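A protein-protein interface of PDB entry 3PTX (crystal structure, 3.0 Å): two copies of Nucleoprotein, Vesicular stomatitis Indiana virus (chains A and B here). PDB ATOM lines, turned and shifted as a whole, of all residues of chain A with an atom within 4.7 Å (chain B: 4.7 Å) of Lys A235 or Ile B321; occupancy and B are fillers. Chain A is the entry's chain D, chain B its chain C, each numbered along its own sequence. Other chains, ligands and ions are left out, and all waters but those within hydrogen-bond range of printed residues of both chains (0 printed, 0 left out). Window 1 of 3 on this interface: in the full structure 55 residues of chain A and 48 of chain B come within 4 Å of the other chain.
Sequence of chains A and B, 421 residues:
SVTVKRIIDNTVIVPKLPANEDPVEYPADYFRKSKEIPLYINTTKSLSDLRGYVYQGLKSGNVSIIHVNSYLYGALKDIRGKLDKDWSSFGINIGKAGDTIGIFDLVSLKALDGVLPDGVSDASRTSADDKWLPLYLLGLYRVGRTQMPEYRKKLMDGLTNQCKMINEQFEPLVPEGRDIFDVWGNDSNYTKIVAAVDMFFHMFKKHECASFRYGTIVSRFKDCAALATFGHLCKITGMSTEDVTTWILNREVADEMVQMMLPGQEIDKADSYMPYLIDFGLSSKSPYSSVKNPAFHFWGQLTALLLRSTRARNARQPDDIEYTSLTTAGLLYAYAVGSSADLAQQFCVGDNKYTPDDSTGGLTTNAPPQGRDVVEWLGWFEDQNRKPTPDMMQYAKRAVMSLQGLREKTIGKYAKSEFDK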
ATOM      1  N   GLY A 231     -12.401  17.728 -12.177  1.00  0.00           N
ATOM      2  CA  GLY A 231     -11.368  18.732 -12.343  1.00  0.00           C
ATOM      3  C   GLY A 231     -10.895  18.925 -13.772  1.00  0.00           C
ATOM      4  O   GLY A 231     -10.412  19.991 -14.149  1.00  0.00           O
ATOM      5  N   HIS A 232     -11.026  17.874 -14.569  1.00  0.00           N
ATOM      6  CA  HIS A 232     -10.476  17.852 -15.922  1.00  0.00           C
ATOM      7  C   HIS A 232     -11.465  18.524 -16.843  1.00  0.00           C
ATOM      8  O   HIS A 232     -11.084  19.313 -17.712  1.00  0.00           O
ATOM      9  CB  HIS A 232     -10.218  16.404 -16.359  1.00  0.00           C
ATOM     10  CG  HIS A 232     -10.104  16.210 -17.843  1.00  0.00           C
ATOM     11  ND1 HIS A 232      -9.050  16.698 -18.586  1.00  0.00           N
ATOM     12  CD2 HIS A 232     -10.891  15.534 -18.718  1.00  0.00           C
ATOM     13  CE1 HIS A 232      -9.197  16.343 -19.851  1.00  0.00           C
ATOM     14  NE2 HIS A 232     -10.304  15.631 -19.954  1.00  0.00           N
ATOM     15  N   LEU A 233     -12.738  18.191 -16.636  1.00  0.00           N
ATOM     16  CA  LEU A 233     -13.848  18.839 -17.313  1.00  0.00           C
ATOM     17  C   LEU A 233     -13.723  20.342 -17.126  1.00  0.00           C
ATOM     18  O   LEU A 233     -13.753  21.111 -18.105  1.00  0.00           O
ATOM     19  CB  LEU A 233     -15.173  18.368 -16.715  1.00  0.00           C
ATOM     20  CG  LEU A 233     -16.449  18.810 -17.430  1.00  0.00           C
ATOM     21  CD1 LEU A 233     -16.450  18.316 -18.875  1.00  0.00           C
ATOM     22  CD2 LEU A 233     -17.677  18.313 -16.693  1.00  0.00           C
ATOM     23  N   CYS A 234     -13.583  20.753 -15.862  1.00  0.00           N
ATOM     24  CA  CYS A 234     -13.395  22.154 -15.528  1.00  0.00           C
ATOM     25  C   CYS A 234     -12.273  22.731 -16.364  1.00  0.00           C
ATOM     26  O   CYS A 234     -12.479  23.667 -17.136  1.00  0.00           O
ATOM     27  CB  CYS A 234     -13.045  22.272 -14.060  1.00  0.00           C
ATOM     28  SG  CYS A 234     -14.453  21.993 -12.986  1.00  0.00           S
ATOM     29  N   LYS A 235     -11.090  22.142 -16.212  1.00  0.00           N
ATOM     30  CA  LYS A 235      -9.888  22.577 -16.921  1.00  0.00           C
ATOM     31  C   LYS A 235     -10.047  22.629 -18.432  1.00  0.00           C
ATOM     32  O   LYS A 235      -9.460  23.478 -19.087  1.00  0.00           O
ATOM     33  CB  LYS A 235      -8.707  21.667 -16.575  1.00  0.00           C
ATOM     34  CG  LYS A 235      -7.948  22.087 -15.318  1.00  0.00           C
ATOM     35  CD  LYS A 235      -7.286  23.461 -15.511  1.00  0.00           C
ATOM     36  CE  LYS A 235      -6.900  24.119 -14.173  1.00  0.00           C
ATOM     37  NZ  LYS A 235      -5.945  23.269 -13.387  1.00  0.00           N
ATOM     38  N   ILE A 236     -10.839  21.714 -18.973  1.00  0.00           N
ATOM     39  CA  ILE A 236     -10.944  21.521 -20.409  1.00  0.00           C
ATOM     40  C   ILE A 236     -12.048  22.414 -21.007  1.00  0.00           C
ATOM     41  O   ILE A 236     -12.073  22.701 -22.218  1.00  0.00           O
ATOM     42  CB  ILE A 236     -11.162  20.030 -20.711  1.00  0.00           C
ATOM     43  CG1 ILE A 236     -10.018  19.488 -21.566  1.00  0.00           C
ATOM     44  CG2 ILE A 236     -12.528  19.782 -21.363  1.00  0.00           C
ATOM     45  CD1 ILE A 236     -10.436  19.225 -23.004  1.00  0.00           C
ATOM     46  N   THR A 237     -12.950  22.865 -20.145  1.00  0.00           N
ATOM     47  CA  THR A 237     -13.970  23.814 -20.545  1.00  0.00           C
ATOM     48  C   THR A 237     -13.581  25.170 -20.003  1.00  0.00           C
ATOM     49  O   THR A 237     -14.371  26.123 -20.056  1.00  0.00           O
ATOM     50  CB  THR A 237     -15.350  23.441 -19.979  1.00  0.00           C
ATOM     51  OG1 THR A 237     -15.319  23.487 -18.545  1.00  0.00           O
ATOM     52  CG2 THR A 237     -15.759  22.043 -20.443  1.00  0.00           C
ATOM     53  N   GLY A 238     -12.365  25.255 -19.470  1.00  0.00           N
ATOM     54  CA  GLY A 238     -11.865  26.488 -18.889  1.00  0.00           C
ATOM     55  C   GLY A 238     -12.788  27.069 -17.835  1.00  0.00           C
ATOM     56  O   GLY A 238     -12.394  27.963 -17.096  1.00  0.00           O
ATOM     57  N   ASN B  20      -3.887  22.289  -6.376  1.00  0.00           N
ATOM     58  CA  ASN B  20      -2.833  22.098  -7.370  1.00  0.00           C
ATOM     59  C   ASN B  20      -1.680  23.088  -7.160  1.00  0.00           C
ATOM     60  O   ASN B  20      -1.513  24.035  -7.926  1.00  0.00           O
ATOM     61  CB  ASN B  20      -3.430  22.272  -8.769  1.00  0.00           C
ATOM     62  CG  ASN B  20      -2.812  21.347  -9.789  1.00  0.00           C
ATOM     63  OD1 ASN B  20      -2.156  20.370  -9.435  1.00  0.00           O
ATOM     64  ND2 ASN B  20      -3.027  21.644 -11.067  1.00  0.00           N
ATOM     65  N   PRO B 294       0.740  26.316 -20.309  1.00  0.00           N
ATOM     66  CA  PRO B 294       0.154  25.321 -21.222  1.00  0.00           C
ATOM     67  C   PRO B 294      -0.730  25.970 -22.265  1.00  0.00           C
ATOM     68  O   PRO B 294      -0.655  25.637 -23.448  1.00  0.00           O
ATOM     69  CB  PRO B 294      -0.736  24.474 -20.308  1.00  0.00           C
ATOM     70  CG  PRO B 294      -0.425  24.907 -18.906  1.00  0.00           C
ATOM     71  CD  PRO B 294       0.116  26.286 -18.977  1.00  0.00           C
ATOM     72  N   ALA B 295      -1.585  26.880 -21.806  1.00  0.00           N
ATOM     73  CA  ALA B 295      -2.473  27.596 -22.681  1.00  0.00           C
ATOM     74  C   ALA B 295      -1.644  28.478 -23.573  1.00  0.00           C
ATOM     75  O   ALA B 295      -1.849  28.510 -24.777  1.00  0.00           O
ATOM     76  CB  ALA B 295      -3.428  28.408 -21.886  1.00  0.00           C
ATOM     77  N   PHE B 298       0.258  26.366 -26.162  1.00  0.00           N
ATOM     78  CA  PHE B 298      -0.596  25.807 -27.193  1.00  0.00           C
ATOM     79  C   PHE B 298      -0.930  26.857 -28.231  1.00  0.00           C
ATOM     80  O   PHE B 298      -0.588  26.741 -29.404  1.00  0.00           O
ATOM     81  CB  PHE B 298      -1.885  25.320 -26.557  1.00  0.00           C
ATOM     82  CG  PHE B 298      -2.843  24.692 -27.528  1.00  0.00           C
ATOM     83  CD1 PHE B 298      -4.065  25.276 -27.788  1.00  0.00           C
ATOM     84  CD2 PHE B 298      -2.522  23.506 -28.167  1.00  0.00           C
ATOM     85  CE1 PHE B 298      -4.950  24.690 -28.669  1.00  0.00           C
ATOM     86  CE2 PHE B 298      -3.407  22.924 -29.050  1.00  0.00           C
ATOM     87  CZ  PHE B 298      -4.619  23.516 -29.298  1.00  0.00           C
ATOM     88  N   PRO B 318      -0.404  20.460 -25.069  1.00  0.00           N
ATOM     89  CA  PRO B 318      -0.520  20.424 -23.609  1.00  0.00           C
ATOM     90  C   PRO B 318      -1.891  19.931 -23.217  1.00  0.00           C
ATOM     91  O   PRO B 318      -2.847  20.125 -23.965  1.00  0.00           O
ATOM     92  CB  PRO B 318      -0.366  21.897 -23.200  1.00  0.00           C
ATOM     93  CG  PRO B 318       0.416  22.507 -24.285  1.00  0.00           C
ATOM     94  CD  PRO B 318      -0.097  21.823 -25.539  1.00  0.00           C
ATOM     95  N   ASP B 319      -1.984  19.285 -22.064  1.00  0.00           N
ATOM     96  CA  ASP B 319      -3.258  18.743 -21.621  1.00  0.00           C
ATOM     97  C   ASP B 319      -3.949  19.700 -20.645  1.00  0.00           C
ATOM     98  O   ASP B 319      -3.346  20.680 -20.170  1.00  0.00           O
ATOM     99  CB  ASP B 319      -3.077  17.335 -21.021  1.00  0.00           C
ATOM    100  CG  ASP B 319      -2.438  16.363 -22.004  1.00  0.00           C
ATOM    101  OD1 ASP B 319      -3.167  15.727 -22.807  1.00  0.00           O
ATOM    102  OD2 ASP B 319      -1.192  16.253 -21.982  1.00  0.00           O
ATOM    103  N   ASP B 320      -5.222  19.417 -20.371  1.00  0.00           N
ATOM    104  CA  ASP B 320      -5.987  20.158 -19.374  1.00  0.00           C
ATOM    105  C   ASP B 320      -5.955  21.660 -19.633  1.00  0.00           C
ATOM    106  O   ASP B 320      -5.799  22.460 -18.710  1.00  0.00           O
ATOM    107  CB  ASP B 320      -5.484  19.841 -17.954  1.00  0.00           C
ATOM    108  CG  ASP B 320      -5.895  18.447 -17.477  1.00  0.00           C
ATOM    109  OD1 ASP B 320      -7.023  18.018 -17.790  1.00  0.00           O
ATOM    110  OD2 ASP B 320      -5.098  17.779 -16.782  1.00  0.00           O
ATOM    111  N   ILE B 321      -6.077  22.029 -20.900  1.00  0.00           N
ATOM    112  CA  ILE B 321      -6.301  23.416 -21.279  1.00  0.00           C
ATOM    113  C   ILE B 321      -7.586  23.528 -22.095  1.00  0.00           C
ATOM    114  O   ILE B 321      -8.090  22.548 -22.611  1.00  0.00           O
ATOM    115  CB  ILE B 321      -5.145  24.006 -22.095  1.00  0.00           C
ATOM    116  CG1 ILE B 321      -5.061  23.348 -23.461  1.00  0.00           C
ATOM    117  CG2 ILE B 321      -3.836  23.882 -21.345  1.00  0.00           C
ATOM    118  CD1 ILE B 321      -3.822  23.728 -24.222  1.00  0.00           C
ATOM    119  N   GLU B 322      -8.144  24.718 -22.213  1.00  0.00           N
ATOM    120  CA  GLU B 322      -9.364  24.790 -22.975  1.00  0.00           C
ATOM    121  C   GLU B 322      -9.012  24.815 -24.446  1.00  0.00           C
ATOM    122  O   GLU B 322      -8.638  25.859 -24.982  1.00  0.00           O
ATOM    123  CB  GLU B 322     -10.221  25.980 -22.586  1.00  0.00           C
ATOM    124  CG  GLU B 322     -11.658  25.705 -22.972  1.00  0.00           C
ATOM    125  CD  GLU B 322     -12.607  26.843 -22.668  1.00  0.00           C
ATOM    126  OE1 GLU B 322     -12.308  27.653 -21.762  1.00  0.00           O
ATOM    127  OE2 GLU B 322     -13.661  26.917 -23.343  1.00  0.00           O
ATOM    128  N   TYR B 323      -9.125  23.658 -25.096  1.00  0.00           N
ATOM    129  CA  TYR B 323      -8.658  23.522 -26.473  1.00  0.00           C
ATOM    130  C   TYR B 323      -9.503  24.293 -27.468  1.00  0.00           C
ATOM    131  O   TYR B 323      -9.005  24.739 -28.497  1.00  0.00           O
ATOM    132  CB  TYR B 323      -8.604  22.061 -26.905  1.00  0.00           C
ATOM    133  CG  TYR B 323      -7.650  21.199 -26.130  1.00  0.00           C
ATOM    134  CD1 TYR B 323      -8.088  20.046 -25.521  1.00  0.00           C
ATOM    135  CD2 TYR B 323      -6.316  21.527 -26.016  1.00  0.00           C
ATOM    136  CE1 TYR B 323      -7.237  19.249 -24.805  1.00  0.00           C
ATOM    137  CE2 TYR B 323      -5.440  20.726 -25.304  1.00  0.00           C
ATOM    138  CZ  TYR B 323      -5.907  19.588 -24.693  1.00  0.00           C
ATOM    139  OH  TYR B 323      -5.064  18.765 -23.967  1.00  0.00           O
ATOM    140  N   LEU B 326      -8.808  28.203 -27.315  1.00  0.00           N
ATOM    141  CA  LEU B 326      -7.421  28.473 -27.609  1.00  0.00           C
ATOM    142  C   LEU B 326      -7.223  28.331 -29.104  1.00  0.00           C
ATOM    143  O   LEU B 326      -6.495  29.104 -29.714  1.00  0.00           O
ATOM    144  CB  LEU B 326      -6.533  27.496 -26.855  1.00  0.00           C
ATOM    145  CG  LEU B 326      -5.813  28.003 -25.613  1.00  0.00           C
ATOM    146  CD1 LEU B 326      -6.301  29.366 -25.269  1.00  0.00           C
ATOM    147  CD2 LEU B 326      -6.002  27.054 -24.432  1.00  0.00           C
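Asp B320 touches Lys A235.
Lys A235 touches Ile B321.
Lys A235 touches Glu B322 (O to N, 3.6 Å).
Ile A236 touches Ile B321.
CG of Glu B322 touches O of Ile A236, 3.1 Å away.
CD1 of Ile A236 touches CD1 of Tyr B323 (3.5 Å).
The backbone carbonyl oxygen (O) of Pro B318 is in hydrogen-bond range of the side-chain hydroxyl (OH) of Tyr B323.
The backbone carbonyl oxygen (O) of Leu A233 lies within hydrogen-bond range of the side-chain hydroxyl (OG1) of Thr A237, 2.9 Å away.
O of Cys A234 is in hydrogen-bond range of OG1 of Thr A237.
Of chain A, only Lys A235 (3.5 Å) and Ile A236 (3.7 Å) come within 4 Å of Ile B321.
Of the printed residues of chain B, Gly A238 touches Glu B322 (3.1 Å).
Of the printed residues of chain B, His A232 touches Asp B320 (2.5 Å).
Printed residues of chain A within 4 Å of Asp B320: His A232 and Lys A235.
Gly A231 touches none of the printed residues of chain B.
The nearest printed residue of chain A that does not touch Ile B321 is Thr A237 (5.5 Å).
Of the 8 printed residues of chain A, 5 touch a printed residue of chain B.
Hydrophobic or aromatic side chains of chain A within 4 Å of the printed part of chain B: His A232 and Ile A236.
Hydrophobic or aromatic side chains of chain B within 4 Å of the printed part of chain A: Tyr B323.
Among the printed residues, 9 pairs touch across the chains.
The side-chain carboxylate of Glu B322 sits close to the backbone carbonyl oxygen of Thr A237, at 3.1 Å.
A ring nitrogen (ND1) of His A232 is in hydrogen-bond range of the side-chain carboxylate (OD1) of Asp B320 (2.5 Å).
OE1 of Glu B322 sits close to N of Gly A238 (3.3 Å).
No position is printed for both chains.
Of the 9 pairs that touch across the chains among the printed residues, none has its exchanged pair printed and touching as well.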
